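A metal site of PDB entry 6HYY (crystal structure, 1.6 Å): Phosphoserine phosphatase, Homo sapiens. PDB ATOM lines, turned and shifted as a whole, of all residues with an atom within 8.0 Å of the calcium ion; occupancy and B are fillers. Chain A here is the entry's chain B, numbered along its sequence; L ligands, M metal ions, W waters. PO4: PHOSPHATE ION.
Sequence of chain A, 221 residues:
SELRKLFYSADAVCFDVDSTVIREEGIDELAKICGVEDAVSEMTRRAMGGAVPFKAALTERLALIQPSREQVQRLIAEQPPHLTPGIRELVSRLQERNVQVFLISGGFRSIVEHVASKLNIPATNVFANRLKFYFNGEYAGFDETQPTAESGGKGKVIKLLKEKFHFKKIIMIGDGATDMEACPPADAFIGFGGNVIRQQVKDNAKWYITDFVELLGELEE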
ATOM      1  N   PHE A  15     -17.677  14.443  16.658  1.00  0.00           N
ATOM      2  CA  PHE A  15     -16.671  13.592  17.297  1.00  0.00           C
ATOM      3  C   PHE A  15     -15.276  14.098  17.002  1.00  0.00           C
ATOM      4  O   PHE A  15     -14.923  14.340  15.841  1.00  0.00           O
ATOM      5  CB  PHE A  15     -16.754  12.138  16.820  1.00  0.00           C
ATOM      6  CG  PHE A  15     -17.979  11.397  17.260  1.00  0.00           C
ATOM      7  CD1 PHE A  15     -17.989  10.697  18.467  1.00  0.00           C
ATOM      8  CD2 PHE A  15     -19.110  11.367  16.455  1.00  0.00           C
ATOM      9  CE1 PHE A  15     -19.132   9.981  18.865  1.00  0.00           C
ATOM     10  CE2 PHE A  15     -20.252  10.660  16.864  1.00  0.00           C
ATOM     11  CZ  PHE A  15     -20.265   9.978  18.054  1.00  0.00           C
ATOM     12  N   ASP A  16     -14.476  14.233  18.048  1.00  0.00           N
ATOM     13  CA  ASP A  16     -13.023  14.241  17.937  1.00  0.00           C
ATOM     14  C   ASP A  16     -12.549  12.931  17.299  1.00  0.00           C
ATOM     15  O   ASP A  16     -13.182  11.893  17.448  1.00  0.00           O
ATOM     16  CB  ASP A  16     -12.462  14.433  19.347  1.00  0.00           C
ATOM     17  CG  ASP A  16     -10.974  14.261  19.423  1.00  0.00           C
ATOM     18  OD1 ASP A  16     -10.252  14.912  18.654  1.00  0.00           O
ATOM     19  OD2 ASP A  16     -10.556  13.499  20.298  1.00  0.00           O
ATOM     20  N   VAL A  17     -11.406  12.984  16.612  1.00  0.00           N
ATOM     21  CA  VAL A  17     -10.910  11.784  15.936  1.00  0.00           C
ATOM     22  C   VAL A  17      -9.803  11.093  16.744  1.00  0.00           C
ATOM     23  O   VAL A  17     -10.003   9.979  17.249  1.00  0.00           O
ATOM     24  CB  VAL A  17     -10.466  12.107  14.512  1.00  0.00           C
ATOM     25  CG1 VAL A  17      -9.895  10.858  13.863  1.00  0.00           C
ATOM     26  CG2 VAL A  17     -11.668  12.601  13.695  1.00  0.00           C
ATOM     27  N   ASP A  18      -8.624  11.730  16.868  1.00  0.00           N
ATOM     28  CA  ASP A  18      -7.505  11.085  17.554  1.00  0.00           C
ATOM     29  C   ASP A  18      -7.876  10.742  19.000  1.00  0.00           C
ATOM     30  O   ASP A  18      -8.302  11.609  19.759  1.00  0.00           O
ATOM     31  CB  ASP A  18      -6.295  12.010  17.566  1.00  0.00           C
ATOM     32  CG  ASP A  18      -5.708  12.249  16.186  1.00  0.00           C
ATOM     33  OD1 ASP A  18      -5.884  11.390  15.289  1.00  0.00           O
ATOM     34  OD2 ASP A  18      -5.087  13.308  16.000  1.00  0.00           O
ATOM     35  N   SER A  19      -7.696   9.468  19.359  1.00  0.00           N
ATOM     36  CA  SER A  19      -7.933   8.908  20.684  1.00  0.00           C
ATOM     37  C   SER A  19      -9.411   8.838  21.033  1.00  0.00           C
ATOM     38  O   SER A  19      -9.759   8.383  22.151  1.00  0.00           O
ATOM     39  CB  SER A  19      -7.197   9.686  21.791  1.00  0.00           C
ATOM     40  OG  SER A  19      -5.815   9.755  21.462  1.00  0.00           O
ATOM     41  N   THR A  20     -10.308   9.249  20.134  1.00  0.00           N
ATOM     42  CA  THR A  20     -11.749   9.124  20.365  1.00  0.00           C
ATOM     43  C   THR A  20     -12.374   8.165  19.359  1.00  0.00           C
ATOM     44  O   THR A  20     -12.678   7.029  19.731  1.00  0.00           O
ATOM     45  CB  THR A  20     -12.416  10.504  20.350  1.00  0.00           C
ATOM     46  OG1 THR A  20     -11.851  11.296  21.403  1.00  0.00           O
ATOM     47  CG2 THR A  20     -13.923  10.364  20.563  1.00  0.00           C
ATOM     48  N   VAL A  21     -12.551   8.572  18.091  1.00  0.00           N
ATOM     49  CA  VAL A  21     -13.089   7.661  17.088  1.00  0.00           C
ATOM     50  C   VAL A  21     -12.090   6.560  16.752  1.00  0.00           C
ATOM     51  O   VAL A  21     -12.494   5.423  16.459  1.00  0.00           O
ATOM     52  CB  VAL A  21     -13.518   8.451  15.835  1.00  0.00           C
ATOM     53  CG1 VAL A  21     -13.787   7.530  14.665  1.00  0.00           C
ATOM     54  CG2 VAL A  21     -14.757   9.267  16.156  1.00  0.00           C
ATOM     55  N   ILE A  22     -10.795   6.867  16.775  1.00  0.00           N
ATOM     56  CA  ILE A  22      -9.736   5.891  16.558  1.00  0.00           C
ATOM     57  C   ILE A  22      -8.905   5.784  17.840  1.00  0.00           C
ATOM     58  O   ILE A  22      -8.890   6.693  18.677  1.00  0.00           O
ATOM     59  CB  ILE A  22      -8.831   6.262  15.359  1.00  0.00           C
ATOM     60  CG1 ILE A  22      -8.267   7.678  15.505  1.00  0.00           C
ATOM     61  CG2 ILE A  22      -9.607   6.119  14.054  1.00  0.00           C
ATOM     62  CD1 ILE A  22      -7.156   8.032  14.495  1.00  0.00           C
ATOM     63  N   GLU A  24      -5.587   5.494  17.991  1.00  0.00           N
ATOM     64  CA  GLU A  24      -4.311   6.148  17.793  1.00  0.00           C
ATOM     65  C   GLU A  24      -4.475   7.651  17.605  1.00  0.00           C
ATOM     66  O   GLU A  24      -5.589   8.190  17.549  1.00  0.00           O
ATOM     67  CB  GLU A  24      -3.605   5.515  16.603  1.00  0.00           C
ATOM     68  CG  GLU A  24      -3.334   4.020  16.772  1.00  0.00           C
ATOM     69  CD  GLU A  24      -4.416   3.129  16.194  1.00  0.00           C
ATOM     70  OE1 GLU A  24      -5.543   3.597  15.903  1.00  0.00           O
ATOM     71  OE2 GLU A  24      -4.138   1.918  16.022  1.00  0.00           O
ATOM     72  N   GLU A  25      -3.351   8.355  17.495  1.00  0.00           N
ATOM     73  CA  GLU A  25      -3.300   9.728  17.014  1.00  0.00           C
ATOM     74  C   GLU A  25      -2.592   9.728  15.672  1.00  0.00           C
ATOM     75  O   GLU A  25      -1.489   9.162  15.549  1.00  0.00           O
ATOM     76  CB  GLU A  25      -2.594  10.646  18.011  1.00  0.00           C
ATOM     77  CG  GLU A  25      -3.038  10.421  19.450  1.00  0.00           C
ATOM     78  CD  GLU A  25      -2.547  11.504  20.392  1.00  0.00           C
ATOM     79  OE1 GLU A  25      -2.262  11.175  21.565  1.00  0.00           O
ATOM     80  OE2 GLU A  25      -2.471  12.675  19.974  1.00  0.00           O
ATOM     81  N   ILE A 104     -14.394  16.330  13.750  1.00  0.00           N
ATOM     82  CA  ILE A 104     -13.622  17.560  13.893  1.00  0.00           C
ATOM     83  C   ILE A 104     -12.269  17.207  14.500  1.00  0.00           C
ATOM     84  O   ILE A 104     -12.202  16.712  15.630  1.00  0.00           O
ATOM     85  CB  ILE A 104     -14.329  18.584  14.790  1.00  0.00           C
ATOM     86  CG1 ILE A 104     -15.747  18.895  14.299  1.00  0.00           C
ATOM     87  CG2 ILE A 104     -13.514  19.887  14.830  1.00  0.00           C
ATOM     88  CD1 ILE A 104     -16.456  19.881  15.223  1.00  0.00           C
ATOM     89  N   SER A 105     -11.184  17.495  13.772  1.00  0.00           N
ATOM     90  CA  SER A 105      -9.874  17.001  14.164  1.00  0.00           C
ATOM     91  C   SER A 105      -8.772  18.033  13.910  1.00  0.00           C
ATOM     92  O   SER A 105      -8.782  18.733  12.893  1.00  0.00           O
ATOM     93  CB  SER A 105      -9.550  15.708  13.410  1.00  0.00           C
ATOM     94  OG  SER A 105      -8.284  15.169  13.772  1.00  0.00           O
ATOM     95  N   GLY A 106      -7.811  18.098  14.838  1.00  0.00           N
ATOM     96  CA  GLY A 106      -6.547  18.753  14.554  1.00  0.00           C
ATOM     97  C   GLY A 106      -5.596  17.919  13.723  1.00  0.00           C
ATOM     98  O   GLY A 106      -4.488  18.369  13.406  1.00  0.00           O
ATOM     99  N   LYS A 154     -11.856  24.036  17.394  1.00  0.00           N
ATOM    100  CA  LYS A 154     -13.047  23.196  17.367  1.00  0.00           C
ATOM    101  C   LYS A 154     -14.292  23.988  17.771  1.00  0.00           C
ATOM    102  O   LYS A 154     -15.354  23.825  17.163  1.00  0.00           O
ATOM    103  CB  LYS A 154     -12.861  21.974  18.255  1.00  0.00           C
ATOM    104  CG  LYS A 154     -11.712  21.106  17.768  1.00  0.00           C
ATOM    105  CD  LYS A 154     -11.839  19.701  18.287  1.00  0.00           C
ATOM    106  CE  LYS A 154     -10.563  18.933  17.946  1.00  0.00           C
ATOM    107  NZ  LYS A 154     -10.674  17.508  18.315  1.00  0.00           N
ATOM    108  N   MET A 172     -20.616  17.839  21.462  1.00  0.00           N
ATOM    109  CA  MET A 172     -19.213  17.579  21.151  1.00  0.00           C
ATOM    110  C   MET A 172     -18.730  16.417  22.008  1.00  0.00           C
ATOM    111  O   MET A 172     -18.977  16.402  23.215  1.00  0.00           O
ATOM    112  CB  MET A 172     -18.352  18.818  21.432  1.00  0.00           C
ATOM    113  CG  MET A 172     -16.845  18.575  21.202  1.00  0.00           C
ATOM    114  SD  MET A 172     -16.487  18.684  19.442  1.00  0.00           S
ATOM    115  CE  MET A 172     -15.319  17.339  19.240  1.00  0.00           C
ATOM    116  N   ILE A 173     -18.043  15.445  21.397  1.00  0.00           N
ATOM    117  CA  ILE A 173     -17.547  14.276  22.131  1.00  0.00           C
ATOM    118  C   ILE A 173     -16.061  14.129  21.850  1.00  0.00           C
ATOM    119  O   ILE A 173     -15.659  14.017  20.688  1.00  0.00           O
ATOM    120  CB  ILE A 173     -18.284  12.984  21.719  1.00  0.00           C
ATOM    121  CG1 ILE A 173     -19.788  13.149  21.956  1.00  0.00           C
ATOM    122  CG2 ILE A 173     -17.699  11.762  22.455  1.00  0.00           C
ATOM    123  CD1 ILE A 173     -20.662  11.934  21.624  1.00  0.00           C
ATOM    124  N   GLY A 174     -15.238  14.131  22.913  1.00  0.00           N
ATOM    125  CA  GLY A 174     -13.808  13.972  22.688  1.00  0.00           C
ATOM    126  C   GLY A 174     -13.045  13.776  23.975  1.00  0.00           C
ATOM    127  O   GLY A 174     -13.594  13.859  25.075  1.00  0.00           O
ATOM    128  N   ASP A 175     -11.742  13.497  23.822  1.00  0.00           N
ATOM    129  CA  ASP A 175     -10.929  13.179  24.983  1.00  0.00           C
ATOM    130  C   ASP A 175     -10.224  14.388  25.576  1.00  0.00           C
ATOM    131  O   ASP A 175      -9.757  14.308  26.716  1.00  0.00           O
ATOM    132  CB  ASP A 175      -9.870  12.132  24.618  1.00  0.00           C
ATOM    133  CG  ASP A 175      -8.840  12.672  23.646  1.00  0.00           C
ATOM    134  OD1 ASP A 175      -9.208  12.944  22.498  1.00  0.00           O
ATOM    135  OD2 ASP A 175      -7.656  12.780  24.028  1.00  0.00           O
ATOM    136  N   GLY A 176     -10.129  15.512  24.857  1.00  0.00           N
ATOM    137  CA  GLY A 176      -9.139  16.527  25.151  1.00  0.00           C
ATOM    138  C   GLY A 176      -9.706  17.883  25.540  1.00  0.00           C
ATOM    139  O   GLY A 176     -10.917  18.137  25.502  1.00  0.00           O
ATOM    140  N   ALA A 177      -8.772  18.771  25.923  1.00  0.00           N
ATOM    141  CA  ALA A 177      -9.094  20.151  26.270  1.00  0.00           C
ATOM    142  C   ALA A 177      -9.681  20.913  25.091  1.00  0.00           C
ATOM    143  O   ALA A 177     -10.584  21.744  25.273  1.00  0.00           O
ATOM    144  CB  ALA A 177      -7.838  20.850  26.767  1.00  0.00           C
ATOM    145  N   THR A 178      -9.155  20.688  23.885  1.00  0.00           N
ATOM    146  CA  THR A 178      -9.681  21.375  22.712  1.00  0.00           C
ATOM    147  C   THR A 178     -11.102  20.940  22.422  1.00  0.00           C
ATOM    148  O   THR A 178     -11.878  21.715  21.840  1.00  0.00           O
ATOM    149  CB  THR A 178      -8.783  21.138  21.496  1.00  0.00           C
ATOM    150  OG1 THR A 178      -8.718  19.738  21.185  1.00  0.00           O
ATOM    151  CG2 THR A 178      -7.379  21.660  21.762  1.00  0.00           C
ATOM    152  N   ASP A 179     -11.480  19.731  22.842  1.00  0.00           N
ATOM    153  CA  ASP A 179     -12.859  19.296  22.695  1.00  0.00           C
ATOM    154  C   ASP A 179     -13.763  19.904  23.756  1.00  0.00           C
ATOM    155  O   ASP A 179     -14.853  20.397  23.437  1.00  0.00           O
ATOM    156  CB  ASP A 179     -12.913  17.761  22.733  1.00  0.00           C
ATOM    157  CG  ASP A 179     -11.906  17.143  21.789  1.00  0.00           C
ATOM    158  OD1 ASP A 179     -12.015  17.420  20.576  1.00  0.00           O
ATOM    159  OD2 ASP A 179     -10.997  16.401  22.236  1.00  0.00           O
ATOM    160  N   PHE A 192     -14.439  11.609  26.625  1.00  0.00           N
ATOM    161  CA  PHE A 192     -14.226  10.211  26.287  1.00  0.00           C
ATOM    162  C   PHE A 192     -12.843   9.758  26.711  1.00  0.00           C
ATOM    163  O   PHE A 192     -11.840  10.255  26.184  1.00  0.00           O
ATOM    164  CB  PHE A 192     -14.402   9.945  24.787  1.00  0.00           C
ATOM    165  CG  PHE A 192     -14.314   8.491  24.457  1.00  0.00           C
ATOM    166  CD1 PHE A 192     -15.341   7.636  24.828  1.00  0.00           C
ATOM    167  CD2 PHE A 192     -13.191   7.970  23.839  1.00  0.00           C
ATOM    168  CE1 PHE A 192     -15.253   6.285  24.566  1.00  0.00           C
ATOM    169  CE2 PHE A 192     -13.078   6.621  23.582  1.00  0.00           C
ATOM    170  CZ  PHE A 192     -14.124   5.770  23.941  1.00  0.00           C
ATOM    171  N   VAL A 196      -7.423   7.649  26.067  1.00  0.00           N
ATOM    172  CA  VAL A 196      -6.585   8.590  26.791  1.00  0.00           C
ATOM    173  C   VAL A 196      -7.449   9.251  27.855  1.00  0.00           C
ATOM    174  O   VAL A 196      -8.536   9.763  27.557  1.00  0.00           O
ATOM    175  CB  VAL A 196      -5.968   9.657  25.864  1.00  0.00           C
ATOM    176  CG1 VAL A 196      -5.119  10.648  26.676  1.00  0.00           C
ATOM    177  CG2 VAL A 196      -5.104   9.005  24.810  1.00  0.00           C
ATOM    178  N   ARG A 198      -7.404  12.346  30.290  1.00  0.00           N
ATOM    179  CA  ARG A 198      -6.802  13.630  30.607  1.00  0.00           C
ATOM    180  C   ARG A 198      -7.444  14.111  31.906  1.00  0.00           C
ATOM    181  O   ARG A 198      -8.662  14.279  31.970  1.00  0.00           O
ATOM    182  CB  ARG A 198      -7.015  14.633  29.470  1.00  0.00           C
ATOM    183  CG  ARG A 198      -6.157  14.329  28.254  1.00  0.00           C
ATOM    184  CD  ARG A 198      -6.523  15.151  27.032  1.00  0.00           C
ATOM    185  NE  ARG A 198      -6.194  14.443  25.798  1.00  0.00           N
ATOM    186  CZ  ARG A 198      -4.982  14.405  25.268  1.00  0.00           C
ATOM    187  NH1 ARG A 198      -3.981  15.067  25.848  1.00  0.00           N
ATOM    188  NH2 ARG A 198      -4.754  13.720  24.151  1.00  0.00           N
HETATM  189  P   PO4 L   1      -7.614  15.457  17.243  1.00  0.00           P
HETATM  190  O1  PO4 L   1      -8.236  16.818  17.388  1.00  0.00           O
HETATM  191  O2  PO4 L   1      -7.311  14.883  18.637  1.00  0.00           O
HETATM  192  O3  PO4 L   1      -6.281  15.673  16.526  1.00  0.00           O
HETATM  193  O4  PO4 L   1      -8.451  14.525  16.402  1.00  0.00           O
HETATM  194 CA    CA M   1      -8.329  13.788  20.529  1.00  0.00          CA
HETATM  195  O   HOH W   1      -6.204  13.258  21.354  1.00  0.00           O
HETATM  196  O   HOH W   2      -8.533  16.073  21.265  1.00  0.00           O
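Three residues have an atom within 4 Å of the calcium ion: Asp 16, Asp 18 and Asp 175.
Along chain A the residues within 4 Å of the calcium ion span positions 16 to 175.
The nearest printed residue that does not touch the calcium ion is Asp 179 (4.1 Å).
Water W2 lies within hydrogen-bond range of OD2 of Asp 179 and OD1 of Asp 16.
Water W1 lies within hydrogen-bond range of OD2 of Asp 175 (3.1 Å) and NH2 of Arg 198 (3.2 Å).
The calcium ion is bound by OD2 of Asp 16, O of Asp 18, OD1 of Asp 175, water W1, water W2 and O2 of the ligand.
The calcium ion has six donor atoms within binding distance.
Slightly farther from the calcium ion lies OD1 of Asp 16 (2.9 Å).
OD2 of Asp 179 sits at hydrogen-bond distance from N of Asp 175, 3.4 Å away.
The side-chain carboxylate of Asp 16 lies within salt-bridge range of the side-chain amino group of Lys 154.
OD2 of Asp 175 lies within salt-bridge range of NE of Arg 198.
O of Asp 16 sits close to N of Val 21, 3.4 Å away.
The side-chain carboxylate of Asp 16 sits close to the side-chain hydroxyl of Thr 20 (2.8 Å).
OG1 of Thr 20 lies within hydrogen-bond range of N of Asp 175 (3.3 Å).
The backbone NH of Asp 16 is in hydrogen-bond range of the backbone carbonyl oxygen of Ile 173, at 2.9 Å.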
